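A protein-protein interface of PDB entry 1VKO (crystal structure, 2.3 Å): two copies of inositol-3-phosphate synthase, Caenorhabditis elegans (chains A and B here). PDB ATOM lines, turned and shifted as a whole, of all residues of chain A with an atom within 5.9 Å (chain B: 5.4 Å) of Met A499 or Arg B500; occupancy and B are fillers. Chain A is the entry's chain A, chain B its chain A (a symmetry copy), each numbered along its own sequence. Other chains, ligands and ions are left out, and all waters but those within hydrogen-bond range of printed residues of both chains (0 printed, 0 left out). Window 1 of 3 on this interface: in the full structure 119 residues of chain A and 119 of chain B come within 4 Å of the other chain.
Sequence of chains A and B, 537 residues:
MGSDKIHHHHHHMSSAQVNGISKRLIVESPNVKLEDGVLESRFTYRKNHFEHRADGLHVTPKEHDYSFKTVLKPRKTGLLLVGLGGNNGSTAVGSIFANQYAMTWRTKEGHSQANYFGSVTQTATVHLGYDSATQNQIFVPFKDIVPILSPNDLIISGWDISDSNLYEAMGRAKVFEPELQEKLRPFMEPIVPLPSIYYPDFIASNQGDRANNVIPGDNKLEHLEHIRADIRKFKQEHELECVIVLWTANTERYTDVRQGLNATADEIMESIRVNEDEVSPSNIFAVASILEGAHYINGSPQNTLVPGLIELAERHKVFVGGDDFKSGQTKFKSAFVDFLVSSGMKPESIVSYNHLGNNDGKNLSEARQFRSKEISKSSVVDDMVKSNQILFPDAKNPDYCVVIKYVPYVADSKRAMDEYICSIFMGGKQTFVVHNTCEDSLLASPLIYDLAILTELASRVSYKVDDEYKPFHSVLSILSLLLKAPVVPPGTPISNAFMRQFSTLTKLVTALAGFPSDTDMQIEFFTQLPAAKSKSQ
OG of Ser A334 lies within hydrogen-bond range of N of Phe A498, 3.2 Å away. The backbone carbonyl oxygen (O) of Met A499 sits at hydrogen-bond distance from the side-chain hydroxyl (OG) of Ser A503, at 3.3 Å. The backbone carbonyl oxygen (O) of Arg A500 lies within hydrogen-bond range of the side-chain hydroxyl (OG1) of Thr A504, 3.1 Å away. The side-chain hydroxyl (OG) of Ser B503 is in hydrogen-bond range of the backbone carbonyl oxygen (O) of Met B499, at 3.3 Å. O of Arg B500 lies within hydrogen-bond range of OG of Ser B503 (3.3 Å). O of Arg B500 lies within hydrogen-bond range of OG1 of Thr B504, 3.1 Å away.
Among the printed residues, merely in contact across the chains: Ala A335 with Phe B339 (3.7 Å), Phe A498 with Phe B339 (3.6 Å), Met A499 with Phe B339 (3.7 Å), Met A499 with Ser B342 (3.3 Å), Met A499 with Arg B500 (3.6 Å), Arg A500 with Met B499 (3.6 Å), Phe A502 with Ser B342 (3.8 Å), Asp A520 with Arg B500 (3.97 Å) and Asp A520 with Ser B503 (3.9 Å).
Ser A334 touches none of the printed residues of chain B. Printed residues of chain B within 4 Å of Phe A498: Phe B339 (3.6 Å). Met A499 touches three residues of chain B. Of the printed residues of chain B, Phe A502 touches Ser B342. Printed residues of chain B within 4 Å of Asp A520: Arg B500 (3.97 Å), Ser B503 (3.9 Å) and Thr B504 (2.9 Å). Of the printed residues of chain A, Phe B339 touches Ala A335 (3.7 Å), Phe A498 (3.6 Å) and Met A499 (3.7 Å). Of the printed residues of chain A, Ser B342 touches Met A499 and Phe A502. Printed residues of chain A within 4 Å of Arg B500: Met A499 (3.6 Å) and Asp A520 (3.97 Å). The nearest residue of chain B that does not touch Met A499 is Asp B338 (4.02 Å).
O of Asp A520 is in hydrogen-bond range of OG1 of Thr B504.
Met A499 touches Arg B500, and with the chains exchanged Arg A500 touches Met B499. Positions printed for both chains: 338, 497, 498, 499, 500, 501, 502, 503 and 504.
Hydrophobic or aromatic side chains of chain B within 4 Å of the printed part of chain A: Phe B339 and Met B499. Printed residues of chain A that touch a printed residue of chain B: Ala A335, Phe A498, Met A499, Arg A500, Phe A502 and Asp A520. Among the printed residues, 10 pairs touch across the chains.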
ATOM      1  N   PHE A 139     -27.316  12.903 -24.855  1.00  0.00           N
ATOM      2  CA  PHE A 139     -26.662  13.092 -23.583  1.00  0.00           C
ATOM      3  C   PHE A 139     -26.794  14.548 -23.160  1.00  0.00           C
ATOM      4  O   PHE A 139     -26.423  15.453 -23.900  1.00  0.00           O
ATOM      5  CB  PHE A 139     -25.192  12.698 -23.713  1.00  0.00           C
ATOM      6  CG  PHE A 139     -24.953  11.204 -23.641  1.00  0.00           C
ATOM      7  CD1 PHE A 139     -24.708  10.575 -22.411  1.00  0.00           C
ATOM      8  CD2 PHE A 139     -24.944  10.428 -24.798  1.00  0.00           C
ATOM      9  CE1 PHE A 139     -24.479   9.199 -22.336  1.00  0.00           C
ATOM     10  CE2 PHE A 139     -24.714   9.041 -24.730  1.00  0.00           C
ATOM     11  CZ  PHE A 139     -24.497   8.439 -23.498  1.00  0.00           C
ATOM     12  N   SER A 334     -13.481   1.760  -5.898  1.00  0.00           N
ATOM     13  CA  SER A 334     -14.945   1.706  -5.987  1.00  0.00           C
ATOM     14  C   SER A 334     -15.506   1.245  -7.341  1.00  0.00           C
ATOM     15  O   SER A 334     -16.368   0.375  -7.382  1.00  0.00           O
ATOM     16  CB  SER A 334     -15.525   3.079  -5.650  1.00  0.00           C
ATOM     17  OG  SER A 334     -16.733   2.922  -4.950  1.00  0.00           O
ATOM     18  N   ALA A 335     -15.028   1.824  -8.437  1.00  0.00           N
ATOM     19  CA  ALA A 335     -15.502   1.413  -9.758  1.00  0.00           C
ATOM     20  C   ALA A 335     -14.868   0.098 -10.296  1.00  0.00           C
ATOM     21  O   ALA A 335     -15.518  -0.610 -11.090  1.00  0.00           O
ATOM     22  CB  ALA A 335     -15.330   2.528 -10.751  1.00  0.00           C
ATOM     23  N   ASP A 338     -16.092  -3.360  -8.512  1.00  0.00           N
ATOM     24  CA  ASP A 338     -17.441  -3.592  -9.085  1.00  0.00           C
ATOM     25  C   ASP A 338     -17.360  -4.235 -10.490  1.00  0.00           C
ATOM     26  O   ASP A 338     -17.916  -5.336 -10.744  1.00  0.00           O
ATOM     27  CB  ASP A 338     -18.193  -2.249  -9.185  1.00  0.00           C
ATOM     28  CG  ASP A 338     -19.713  -2.403  -9.412  1.00  0.00           C
ATOM     29  OD1 ASP A 338     -20.415  -3.074  -8.614  1.00  0.00           O
ATOM     30  OD2 ASP A 338     -20.301  -1.828 -10.342  1.00  0.00           O
ATOM     31  N   ALA A 497     -20.274   0.944  -4.591  1.00  0.00           N
ATOM     32  CA  ALA A 497     -19.761   0.901  -5.952  1.00  0.00           C
ATOM     33  C   ALA A 497     -20.180   2.148  -6.709  1.00  0.00           C
ATOM     34  O   ALA A 497     -21.369   2.368  -6.972  1.00  0.00           O
ATOM     35  CB  ALA A 497     -20.212  -0.356  -6.657  1.00  0.00           C
ATOM     36  N   PHE A 498     -19.180   2.950  -7.062  1.00  0.00           N
ATOM     37  CA  PHE A 498     -19.369   4.297  -7.597  1.00  0.00           C
ATOM     38  C   PHE A 498     -20.368   4.410  -8.738  1.00  0.00           C
ATOM     39  O   PHE A 498     -21.291   5.214  -8.662  1.00  0.00           O
ATOM     40  CB  PHE A 498     -18.025   4.904  -8.018  1.00  0.00           C
ATOM     41  CG  PHE A 498     -18.146   6.221  -8.763  1.00  0.00           C
ATOM     42  CD1 PHE A 498     -18.198   7.433  -8.068  1.00  0.00           C
ATOM     43  CD2 PHE A 498     -18.192   6.249 -10.153  1.00  0.00           C
ATOM     44  CE1 PHE A 498     -18.301   8.656  -8.751  1.00  0.00           C
ATOM     45  CE2 PHE A 498     -18.290   7.471 -10.839  1.00  0.00           C
ATOM     46  CZ  PHE A 498     -18.346   8.674 -10.137  1.00  0.00           C
ATOM     47  N   MET A 499     -20.187   3.638  -9.802  1.00  0.00           N
ATOM     48  CA  MET A 499     -21.072   3.796 -10.951  1.00  0.00           C
ATOM     49  C   MET A 499     -22.531   3.485 -10.567  1.00  0.00           C
ATOM     50  O   MET A 499     -23.477   4.082 -11.095  1.00  0.00           O
ATOM     51  CB  MET A 499     -20.560   3.006 -12.173  1.00  0.00           C
ATOM     52  CG  MET A 499     -19.236   3.580 -12.799  1.00  0.00           C
ATOM     53  SD  MET A 499     -19.259   5.343 -13.334  1.00  0.00           S
ATOM     54  CE  MET A 499     -20.675   5.397 -14.460  1.00  0.00           C
ATOM     55  N   ARG A 500     -22.706   2.613  -9.584  1.00  0.00           N
ATOM     56  CA  ARG A 500     -24.025   2.303  -9.079  1.00  0.00           C
ATOM     57  C   ARG A 500     -24.620   3.515  -8.318  1.00  0.00           C
ATOM     58  O   ARG A 500     -25.840   3.780  -8.372  1.00  0.00           O
ATOM     59  CB  ARG A 500     -23.943   1.049  -8.206  1.00  0.00           C
ATOM     60  CG  ARG A 500     -23.172  -0.128  -8.854  1.00  0.00           C
ATOM     61  CD  ARG A 500     -24.043  -1.278  -9.388  1.00  0.00           C
ATOM     62  NE  ARG A 500     -23.305  -2.548  -9.458  1.00  0.00           N
ATOM     63  CZ  ARG A 500     -23.147  -3.303 -10.558  1.00  0.00           C
ATOM     64  NH1 ARG A 500     -23.686  -2.949 -11.724  1.00  0.00           N
ATOM     65  NH2 ARG A 500     -22.443  -4.431 -10.488  1.00  0.00           N
ATOM     66  N   GLN A 501     -23.740   4.258  -7.645  1.00  0.00           N
ATOM     67  CA  GLN A 501     -24.119   5.436  -6.867  1.00  0.00           C
ATOM     68  C   GLN A 501     -24.484   6.604  -7.767  1.00  0.00           C
ATOM     69  O   GLN A 501     -25.225   7.516  -7.381  1.00  0.00           O
ATOM     70  CB  GLN A 501     -22.964   5.857  -5.943  1.00  0.00           C
ATOM     71  CG  GLN A 501     -22.639   4.908  -4.786  1.00  0.00           C
ATOM     72  CD  GLN A 501     -21.259   5.191  -4.219  1.00  0.00           C
ATOM     73  OE1 GLN A 501     -20.393   5.669  -4.944  1.00  0.00           O
ATOM     74  NE2 GLN A 501     -21.060   4.935  -2.923  1.00  0.00           N
ATOM     75  N   PHE A 502     -23.910   6.590  -8.957  1.00  0.00           N
ATOM     76  CA  PHE A 502     -24.123   7.606  -9.967  1.00  0.00           C
ATOM     77  C   PHE A 502     -25.476   7.381 -10.646  1.00  0.00           C
ATOM     78  O   PHE A 502     -26.216   8.338 -10.898  1.00  0.00           O
ATOM     79  CB  PHE A 502     -22.952   7.557 -10.951  1.00  0.00           C
ATOM     80  CG  PHE A 502     -23.109   8.429 -12.166  1.00  0.00           C
ATOM     81  CD1 PHE A 502     -22.839   9.793 -12.109  1.00  0.00           C
ATOM     82  CD2 PHE A 502     -23.458   7.865 -13.401  1.00  0.00           C
ATOM     83  CE1 PHE A 502     -22.963  10.605 -13.250  1.00  0.00           C
ATOM     84  CE2 PHE A 502     -23.579   8.666 -14.549  1.00  0.00           C
ATOM     85  CZ  PHE A 502     -23.323  10.038 -14.462  1.00  0.00           C
ATOM     86  N   SER A 503     -25.821   6.124 -10.921  1.00  0.00           N
ATOM     87  CA  SER A 503     -27.118   5.864 -11.524  1.00  0.00           C
ATOM     88  C   SER A 503     -28.265   6.120 -10.580  1.00  0.00           C
ATOM     89  O   SER A 503     -29.344   6.515 -11.027  1.00  0.00           O
ATOM     90  CB  SER A 503     -27.205   4.514 -12.249  1.00  0.00           C
ATOM     91  OG  SER A 503     -26.663   3.445 -11.501  1.00  0.00           O
ATOM     92  N   THR A 504     -28.031   5.993  -9.276  1.00  0.00           N
ATOM     93  CA  THR A 504     -29.033   6.406  -8.272  1.00  0.00           C
ATOM     94  C   THR A 504     -29.331   7.898  -8.444  1.00  0.00           C
ATOM     95  O   THR A 504     -30.486   8.303  -8.564  1.00  0.00           O
ATOM     96  CB  THR A 504     -28.518   6.151  -6.871  1.00  0.00           C
ATOM     97  OG1 THR A 504     -28.263   4.741  -6.698  1.00  0.00           O
ATOM     98  CG2 THR A 504     -29.570   6.452  -5.855  1.00  0.00           C
ATOM     99  N   ASP A 520     -30.883   2.044 -20.255  1.00  0.00           N
ATOM    100  CA  ASP A 520     -29.745   1.108 -20.021  1.00  0.00           C
ATOM    101  C   ASP A 520     -29.944  -0.178 -20.807  1.00  0.00           C
ATOM    102  O   ASP A 520     -29.049  -1.000 -20.896  1.00  0.00           O
ATOM    103  CB  ASP A 520     -29.476   0.834 -18.526  1.00  0.00           C
ATOM    104  CG  ASP A 520     -30.648   0.149 -17.798  1.00  0.00           C
ATOM    105  OD1 ASP A 520     -31.797   0.329 -18.181  1.00  0.00           O
ATOM    106  OD2 ASP A 520     -30.521  -0.598 -16.809  1.00  0.00           O
ATOM    107  N   ASP B 338     -15.261   5.036 -19.244  1.00  0.00           N
ATOM    108  CA  ASP B 338     -16.663   5.318 -18.845  1.00  0.00           C
ATOM    109  C   ASP B 338     -16.736   5.960 -17.440  1.00  0.00           C
ATOM    110  O   ASP B 338     -17.280   7.081 -17.255  1.00  0.00           O
ATOM    111  CB  ASP B 338     -17.469   4.003 -18.844  1.00  0.00           C
ATOM    112  CG  ASP B 338     -18.999   4.211 -18.810  1.00  0.00           C
ATOM    113  OD1 ASP B 338     -19.570   4.906 -19.688  1.00  0.00           O
ATOM    114  OD2 ASP B 338     -19.720   3.661 -17.962  1.00  0.00           O
ATOM    115  N   PHE B 339     -16.213   5.226 -16.456  1.00  0.00           N
ATOM    116  CA  PHE B 339     -16.034   5.741 -15.100  1.00  0.00           C
ATOM    117  C   PHE B 339     -15.410   7.162 -15.099  1.00  0.00           C
ATOM    118  O   PHE B 339     -15.908   8.030 -14.394  1.00  0.00           O
ATOM    119  CB  PHE B 339     -15.217   4.765 -14.206  1.00  0.00           C
ATOM    120  CG  PHE B 339     -14.427   5.466 -13.116  1.00  0.00           C
ATOM    121  CD1 PHE B 339     -15.071   5.989 -11.983  1.00  0.00           C
ATOM    122  CD2 PHE B 339     -13.047   5.652 -13.237  1.00  0.00           C
ATOM    123  CE1 PHE B 339     -14.347   6.671 -10.976  1.00  0.00           C
ATOM    124  CE2 PHE B 339     -12.315   6.326 -12.231  1.00  0.00           C
ATOM    125  CZ  PHE B 339     -12.970   6.842 -11.107  1.00  0.00           C
ATOM    126  N   SER B 342     -17.885   9.852 -16.849  1.00  0.00           N
ATOM    127  CA  SER B 342     -18.985   9.987 -15.896  1.00  0.00           C
ATOM    128  C   SER B 342     -18.595  10.837 -14.668  1.00  0.00           C
ATOM    129  O   SER B 342     -19.405  11.634 -14.185  1.00  0.00           O
ATOM    130  CB  SER B 342     -19.496   8.612 -15.447  1.00  0.00           C
ATOM    131  OG  SER B 342     -20.149   7.937 -16.502  1.00  0.00           O
ATOM    132  N   MET B 384     -18.226   7.386 -25.961  1.00  0.00           N
ATOM    133  CA  MET B 384     -18.017   8.130 -24.709  1.00  0.00           C
ATOM    134  C   MET B 384     -17.560   9.599 -24.926  1.00  0.00           C
ATOM    135  O   MET B 384     -18.019  10.513 -24.234  1.00  0.00           O
ATOM    136  CB  MET B 384     -17.071   7.366 -23.758  1.00  0.00           C
ATOM    137  CG  MET B 384     -17.776   6.592 -22.618  1.00  0.00           C
ATOM    138  SD  MET B 384     -18.397   7.611 -21.230  1.00  0.00           S
ATOM    139  CE  MET B 384     -20.182   7.630 -21.477  1.00  0.00           C
ATOM    140  N   SER B 495     -22.174   0.547 -28.877  1.00  0.00           N
ATOM    141  CA  SER B 495     -22.105   0.842 -27.450  1.00  0.00           C
ATOM    142  C   SER B 495     -20.885   0.148 -26.863  1.00  0.00           C
ATOM    143  O   SER B 495     -20.846  -1.094 -26.814  1.00  0.00           O
ATOM    144  CB  SER B 495     -23.392   0.376 -26.755  1.00  0.00           C
ATOM    145  OG  SER B 495     -23.429   0.836 -25.420  1.00  0.00           O
ATOM    146  N   ALA B 497     -19.068   0.876 -23.671  1.00  0.00           N
ATOM    147  CA  ALA B 497     -18.729   0.903 -22.256  1.00  0.00           C
ATOM    148  C   ALA B 497     -19.284  -0.326 -21.560  1.00  0.00           C
ATOM    149  O   ALA B 497     -20.504  -0.502 -21.450  1.00  0.00           O
ATOM    150  CB  ALA B 497     -19.220   2.178 -21.610  1.00  0.00           C
ATOM    151  N   PHE B 498     -18.367  -1.163 -21.086  1.00  0.00           N
ATOM    152  CA  PHE B 498     -18.670  -2.501 -20.582  1.00  0.00           C
ATOM    153  C   PHE B 498     -19.808  -2.575 -19.577  1.00  0.00           C
ATOM    154  O   PHE B 498     -20.742  -3.345 -19.770  1.00  0.00           O
ATOM    155  CB  PHE B 498     -17.412  -3.155 -19.997  1.00  0.00           C
ATOM    156  CG  PHE B 498     -17.674  -4.464 -19.276  1.00  0.00           C
ATOM    157  CD1 PHE B 498     -17.682  -5.676 -19.974  1.00  0.00           C
ATOM    158  CD2 PHE B 498     -17.895  -4.487 -17.903  1.00  0.00           C
ATOM    159  CE1 PHE B 498     -17.913  -6.892 -19.313  1.00  0.00           C
ATOM    160  CE2 PHE B 498     -18.123  -5.704 -17.238  1.00  0.00           C
ATOM    161  CZ  PHE B 498     -18.133  -6.906 -17.944  1.00  0.00           C
ATOM    162  N   MET B 499     -19.735  -1.807 -18.496  1.00  0.00           N
ATOM    163  CA  MET B 499     -20.763  -1.931 -17.469  1.00  0.00           C
ATOM    164  C   MET B 499     -22.150  -1.569 -18.033  1.00  0.00           C
ATOM    165  O   MET B 499     -23.176  -2.129 -17.629  1.00  0.00           O
ATOM    166  CB  MET B 499     -20.381  -1.157 -16.190  1.00  0.00           C
ATOM    167  CG  MET B 499     -19.168  -1.777 -15.403  1.00  0.00           C
ATOM    168  SD  MET B 499     -19.321  -3.537 -14.879  1.00  0.00           S
ATOM    169  CE  MET B 499     -20.869  -3.537 -13.941  1.00  0.00           C
ATOM    170  N   ARG B 500     -22.168  -0.693 -19.028  1.00  0.00           N
ATOM    171  CA  ARG B 500     -23.400  -0.337 -19.695  1.00  0.00           C
ATOM    172  C   ARG B 500     -23.938  -1.528 -20.527  1.00  0.00           C
ATOM    173  O   ARG B 500     -25.164  -1.749 -20.628  1.00  0.00           O
ATOM    174  CB  ARG B 500     -23.165   0.912 -20.548  1.00  0.00           C
ATOM    175  CG  ARG B 500     -22.439   2.062 -19.804  1.00  0.00           C
ATOM    176  CD  ARG B 500     -23.328   3.244 -19.382  1.00  0.00           C
ATOM    177  NE  ARG B 500     -22.560   4.486 -19.217  1.00  0.00           N
ATOM    178  CZ  ARG B 500     -22.516   5.237 -18.104  1.00  0.00           C
ATOM    179  NH1 ARG B 500     -23.210   4.906 -17.016  1.00  0.00           N
ATOM    180  NH2 ARG B 500     -21.767   6.339 -18.082  1.00  0.00           N
ATOM    181  N   GLN B 501     -23.008  -2.304 -21.085  1.00  0.00           N
ATOM    182  CA  GLN B 501     -23.328  -3.470 -21.908  1.00  0.00           C
ATOM    183  C   GLN B 501     -23.845  -4.622 -21.063  1.00  0.00           C
ATOM    184  O   GLN B 501     -24.563  -5.507 -21.542  1.00  0.00           O
ATOM    185  CB  GLN B 501     -22.082  -3.934 -22.680  1.00  0.00           C
ATOM    186  CG  GLN B 501     -21.579  -3.000 -23.784  1.00  0.00           C
ATOM    187  CD  GLN B 501     -20.150  -3.333 -24.173  1.00  0.00           C
ATOM    188  OE1 GLN B 501     -19.400  -3.841 -23.347  1.00  0.00           O
ATOM    189  NE2 GLN B 501     -19.780  -3.088 -25.433  1.00  0.00           N
ATOM    190  N   PHE B 502     -23.425  -4.625 -19.811  1.00  0.00           N
ATOM    191  CA  PHE B 502     -23.801  -5.630 -18.838  1.00  0.00           C
ATOM    192  C   PHE B 502     -25.220  -5.356 -18.335  1.00  0.00           C
ATOM    193  O   PHE B 502     -26.019  -6.285 -18.180  1.00  0.00           O
ATOM    194  CB  PHE B 502     -22.762  -5.622 -17.714  1.00  0.00           C
ATOM    195  CG  PHE B 502     -23.102  -6.485 -16.530  1.00  0.00           C
ATOM    196  CD1 PHE B 502     -22.876  -7.858 -16.556  1.00  0.00           C
ATOM    197  CD2 PHE B 502     -23.584  -5.906 -15.348  1.00  0.00           C
ATOM    198  CE1 PHE B 502     -23.172  -8.662 -15.441  1.00  0.00           C
ATOM    199  CE2 PHE B 502     -23.876  -6.699 -14.227  1.00  0.00           C
ATOM    200  CZ  PHE B 502     -23.661  -8.080 -14.284  1.00  0.00           C
ATOM    201  N   SER B 503     -25.551  -4.087 -18.103  1.00  0.00           N
ATOM    202  CA  SER B 503     -26.903  -3.779 -17.666  1.00  0.00           C
ATOM    203  C   SER B 503     -27.931  -3.996 -18.748  1.00  0.00           C
ATOM    204  O   SER B 503     -29.071  -4.350 -18.442  1.00  0.00           O
ATOM    205  CB  SER B 503     -27.033  -2.425 -16.955  1.00  0.00           C
ATOM    206  OG  SER B 503     -26.362  -1.378 -17.627  1.00  0.00           O
ATOM    207  N   THR B 504     -27.530  -3.880 -20.012  1.00  0.00           N
ATOM    208  CA  THR B 504     -28.412  -4.259 -21.136  1.00  0.00           C
ATOM    209  C   THR B 504     -28.783  -5.739 -21.006  1.00  0.00           C
ATOM    210  O   THR B 504     -29.957  -6.101 -21.033  1.00  0.00           O
ATOM    211  CB  THR B 504     -27.716  -4.026 -22.460  1.00  0.00           C
ATOM    212  OG1 THR B 504     -27.390  -2.626 -22.597  1.00  0.00           O
ATOM    213  CG2 THR B 504     -28.641  -4.291 -23.601  1.00  0.00           C
